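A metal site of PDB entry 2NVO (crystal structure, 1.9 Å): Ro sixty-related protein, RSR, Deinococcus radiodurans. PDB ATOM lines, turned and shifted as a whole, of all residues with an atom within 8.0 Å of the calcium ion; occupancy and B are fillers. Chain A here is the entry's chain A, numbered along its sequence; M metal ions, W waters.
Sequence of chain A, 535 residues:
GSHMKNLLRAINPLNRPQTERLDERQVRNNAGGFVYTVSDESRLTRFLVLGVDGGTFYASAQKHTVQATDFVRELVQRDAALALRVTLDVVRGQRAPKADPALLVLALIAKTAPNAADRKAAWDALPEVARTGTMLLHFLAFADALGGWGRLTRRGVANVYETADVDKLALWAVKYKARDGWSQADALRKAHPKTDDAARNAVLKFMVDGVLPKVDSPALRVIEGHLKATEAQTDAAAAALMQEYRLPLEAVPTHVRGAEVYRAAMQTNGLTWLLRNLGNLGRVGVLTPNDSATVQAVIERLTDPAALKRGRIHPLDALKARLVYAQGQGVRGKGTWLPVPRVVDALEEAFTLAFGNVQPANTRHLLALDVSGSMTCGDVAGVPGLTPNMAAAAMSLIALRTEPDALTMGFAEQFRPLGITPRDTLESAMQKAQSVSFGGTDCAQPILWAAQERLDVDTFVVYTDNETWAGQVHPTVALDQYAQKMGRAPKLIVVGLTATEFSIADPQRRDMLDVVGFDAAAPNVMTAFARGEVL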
ATOM      1  N   ASP A 370      10.656 -26.105   1.477  1.00  0.00           N
ATOM      2  CA  ASP A 370      11.730 -26.312   0.529  1.00  0.00           C
ATOM      3  C   ASP A 370      13.009 -26.509   1.372  1.00  0.00           C
ATOM      4  O   ASP A 370      13.330 -25.682   2.228  1.00  0.00           O
ATOM      5  CB  ASP A 370      11.829 -25.068  -0.385  1.00  0.00           C
ATOM      6  CG  ASP A 370      12.757 -25.267  -1.582  1.00  0.00           C
ATOM      7  OD1 ASP A 370      13.812 -25.900  -1.422  1.00  0.00           O
ATOM      8  OD2 ASP A 370      12.419 -24.781  -2.684  1.00  0.00           O
ATOM      9  N   VAL A 371      13.708 -27.615   1.164  1.00  0.00           N
ATOM     10  CA  VAL A 371      14.902 -27.934   1.943  1.00  0.00           C
ATOM     11  C   VAL A 371      16.175 -27.997   1.095  1.00  0.00           C
ATOM     12  O   VAL A 371      17.194 -28.498   1.541  1.00  0.00           O
ATOM     13  CB  VAL A 371      14.749 -29.292   2.718  1.00  0.00           C
ATOM     14  CG1 VAL A 371      13.626 -29.196   3.750  1.00  0.00           C
ATOM     15  CG2 VAL A 371      14.494 -30.440   1.745  1.00  0.00           C
ATOM     16  N   SER A 372      16.093 -27.502  -0.131  1.00  0.00           N
ATOM     17  CA  SER A 372      17.242 -27.557  -1.043  1.00  0.00           C
ATOM     18  C   SER A 372      18.258 -26.478  -0.700  1.00  0.00           C
ATOM     19  O   SER A 372      17.967 -25.540   0.050  1.00  0.00           O
ATOM     20  CB  SER A 372      16.772 -27.397  -2.479  1.00  0.00           C
ATOM     21  OG  SER A 372      16.143 -26.150  -2.658  1.00  0.00           O
ATOM     22  N   GLY A 373      19.464 -26.620  -1.275  1.00  0.00           N
ATOM     23  CA  GLY A 373      20.584 -25.758  -0.919  1.00  0.00           C
ATOM     24  C   GLY A 373      20.421 -24.274  -1.161  1.00  0.00           C
ATOM     25  O   GLY A 373      20.978 -23.445  -0.415  1.00  0.00           O
ATOM     26  N   SER A 374      19.669 -23.898  -2.191  1.00  0.00           N
ATOM     27  CA  SER A 374      19.511 -22.479  -2.482  1.00  0.00           C
ATOM     28  C   SER A 374      18.761 -21.758  -1.353  1.00  0.00           C
ATOM     29  O   SER A 374      18.853 -20.535  -1.232  1.00  0.00           O
ATOM     30  CB  SER A 374      18.806 -22.265  -3.823  1.00  0.00           C
ATOM     31  OG  SER A 374      17.463 -22.715  -3.766  1.00  0.00           O
ATOM     32  N   MET A 375      18.060 -22.512  -0.506  1.00  0.00           N
ATOM     33  CA  MET A 375      17.355 -21.907   0.641  1.00  0.00           C
ATOM     34  C   MET A 375      18.361 -21.232   1.586  1.00  0.00           C
ATOM     35  O   MET A 375      17.981 -20.398   2.396  1.00  0.00           O
ATOM     36  CB  MET A 375      16.506 -22.954   1.389  1.00  0.00           C
ATOM     37  CG  MET A 375      15.288 -23.441   0.592  1.00  0.00           C
ATOM     38  SD  MET A 375      14.058 -22.187   0.228  1.00  0.00           S
ATOM     39  CE  MET A 375      13.209 -22.035   1.837  1.00  0.00           C
ATOM     40  N   THR A 376      19.630 -21.617   1.495  1.00  0.00           N
ATOM     41  CA  THR A 376      20.680 -20.990   2.311  1.00  0.00           C
ATOM     42  C   THR A 376      21.242 -19.691   1.681  1.00  0.00           C
ATOM     43  O   THR A 376      22.154 -19.062   2.249  1.00  0.00           O
ATOM     44  CB  THR A 376      21.846 -21.968   2.650  1.00  0.00           C
ATOM     45  OG1 THR A 376      22.604 -22.245   1.468  1.00  0.00           O
ATOM     46  CG2 THR A 376      21.295 -23.263   3.231  1.00  0.00           C
ATOM     47  N   PHE A 438      17.080 -33.551  -2.585  1.00  0.00           N
ATOM     48  CA  PHE A 438      15.800 -32.866  -2.473  1.00  0.00           C
ATOM     49  C   PHE A 438      15.013 -33.186  -3.725  1.00  0.00           C
ATOM     50  O   PHE A 438      15.556 -33.737  -4.675  1.00  0.00           O
ATOM     51  CB  PHE A 438      16.024 -31.360  -2.326  1.00  0.00           C
ATOM     52  CG  PHE A 438      16.846 -30.766  -3.436  1.00  0.00           C
ATOM     53  CD1 PHE A 438      16.266 -30.395  -4.624  1.00  0.00           C
ATOM     54  CD2 PHE A 438      18.220 -30.631  -3.293  1.00  0.00           C
ATOM     55  CE1 PHE A 438      17.022 -29.848  -5.662  1.00  0.00           C
ATOM     56  CE2 PHE A 438      18.996 -30.092  -4.336  1.00  0.00           C
ATOM     57  CZ  PHE A 438      18.391 -29.700  -5.517  1.00  0.00           C
ATOM     58  N   GLY A 439      13.734 -32.844  -3.716  1.00  0.00           N
ATOM     59  CA  GLY A 439      12.892 -32.975  -4.894  1.00  0.00           C
ATOM     60  C   GLY A 439      12.343 -31.625  -5.280  1.00  0.00           C
ATOM     61  O   GLY A 439      12.632 -30.626  -4.631  1.00  0.00           O
ATOM     62  N   THR A 441      10.000 -28.449  -5.742  1.00  0.00           N
ATOM     63  CA  THR A 441       9.107 -27.805  -4.785  1.00  0.00           C
ATOM     64  C   THR A 441       7.676 -27.750  -5.359  1.00  0.00           C
ATOM     65  O   THR A 441       7.236 -26.750  -5.876  1.00  0.00           O
ATOM     66  CB  THR A 441       9.630 -26.437  -4.357  1.00  0.00           C
ATOM     67  OG1 THR A 441      10.876 -26.642  -3.672  1.00  0.00           O
ATOM     68  CG2 THR A 441       8.640 -25.789  -3.380  1.00  0.00           C
ATOM     69  N   THR A 464       9.298 -21.430   0.187  1.00  0.00           N
ATOM     70  CA  THR A 464      10.348 -21.615  -0.808  1.00  0.00           C
ATOM     71  C   THR A 464      11.138 -20.291  -0.954  1.00  0.00           C
ATOM     72  O   THR A 464      10.836 -19.315  -0.274  1.00  0.00           O
ATOM     73  CB  THR A 464       9.786 -22.126  -2.162  1.00  0.00           C
ATOM     74  OG1 THR A 464      10.870 -22.506  -3.032  1.00  0.00           O
ATOM     75  CG2 THR A 464       8.953 -21.082  -2.833  1.00  0.00           C
ATOM     76  N   ASP A 465      12.187 -20.280  -1.765  1.00  0.00           N
ATOM     77  CA  ASP A 465      12.902 -19.021  -1.977  1.00  0.00           C
ATOM     78  C   ASP A 465      12.259 -18.347  -3.172  1.00  0.00           C
ATOM     79  O   ASP A 465      11.410 -17.455  -3.045  1.00  0.00           O
ATOM     80  CB  ASP A 465      14.425 -19.205  -2.129  1.00  0.00           C
ATOM     81  CG  ASP A 465      14.829 -20.445  -2.930  1.00  0.00           C
ATOM     82  OD1 ASP A 465      13.988 -21.083  -3.585  1.00  0.00           O
ATOM     83  OD2 ASP A 465      16.018 -20.794  -2.875  1.00  0.00           O
ATOM     84  N   ASN A 466      12.598 -18.842  -4.357  1.00  0.00           N
ATOM     85  CA  ASN A 466      11.931 -18.401  -5.547  1.00  0.00           C
ATOM     86  C   ASN A 466      11.787 -19.553  -6.558  1.00  0.00           C
ATOM     87  O   ASN A 466      11.861 -19.316  -7.741  1.00  0.00           O
ATOM     88  CB  ASN A 466      12.658 -17.185  -6.129  1.00  0.00           C
ATOM     89  CG  ASN A 466      14.084 -17.499  -6.604  1.00  0.00           C
ATOM     90  OD1 ASN A 466      14.619 -18.579  -6.337  1.00  0.00           O
ATOM     91  ND2 ASN A 466      14.687 -16.549  -7.314  1.00  0.00           N
ATOM     92  N   GLU A 467      11.575 -20.778  -6.087  1.00  0.00           N
ATOM     93  CA  GLU A 467      11.600 -21.932  -6.992  1.00  0.00           C
ATOM     94  C   GLU A 467      10.458 -22.917  -6.841  1.00  0.00           C
ATOM     95  O   GLU A 467      10.694 -24.103  -6.591  1.00  0.00           O
ATOM     96  CB  GLU A 467      12.944 -22.676  -6.888  1.00  0.00           C
ATOM     97  CG  GLU A 467      14.125 -21.817  -7.203  1.00  0.00           C
ATOM     98  CD  GLU A 467      15.376 -22.616  -7.511  1.00  0.00           C
ATOM     99  OE1 GLU A 467      15.998 -22.323  -8.533  1.00  0.00           O
ATOM    100  OE2 GLU A 467      15.750 -23.529  -6.763  1.00  0.00           O
ATOM    101  N   THR A 468       9.227 -22.441  -7.020  1.00  0.00           N
ATOM    102  CA  THR A 468       8.105 -23.346  -7.201  1.00  0.00           C
ATOM    103  C   THR A 468       8.351 -24.131  -8.498  1.00  0.00           C
ATOM    104  O   THR A 468       8.878 -23.611  -9.483  1.00  0.00           O
ATOM    105  CB  THR A 468       6.767 -22.610  -7.294  1.00  0.00           C
ATOM    106  OG1 THR A 468       6.807 -21.678  -8.390  1.00  0.00           O
ATOM    107  CG2 THR A 468       6.457 -21.869  -5.988  1.00  0.00           C
HETATM  108 CA    CA M   1      16.317 -24.716  -4.789  1.00  0.00          CA
HETATM  109  O   HOH W   1      15.039 -26.671  -5.607  1.00  0.00           O
HETATM  110  O   HOH W   2      14.368 -23.556  -3.871  1.00  0.00           O
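The side-chain carboxylate (OD1) of Asp 465 is in hydrogen-bond range of the backbone NH (N) of Glu 467 (3.5 Å).
The side-chain carboxylate of Asp 465 lies close to the side-chain hydroxyl of Ser 374 (2.6 Å).
The backbone NH (N) of Ser 372 lies within hydrogen-bond range of the side-chain carboxylate (OD1) of Asp 370 (3.1 Å).
The nearest printed residue that does not touch the calcium ion is Asp 370 (4.4 Å).
OE2 of Glu 467 is bound to the calcium ion, 2.4 Å away.
Water W2 binds the calcium ion.
Water W1 is bound to the calcium ion (2.5 Å).
The calcium ion is bound by OG of Ser 374 (2.5 Å).
The calcium ion is bound by the side-chain hydroxyl (OG) of Ser 372, 2.6 Å away.
Water W2 lies within hydrogen-bond range of the side-chain carboxylate of Asp 465 (2.5 Å) and the side-chain carboxylate of Asp 370 (2.6 Å).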
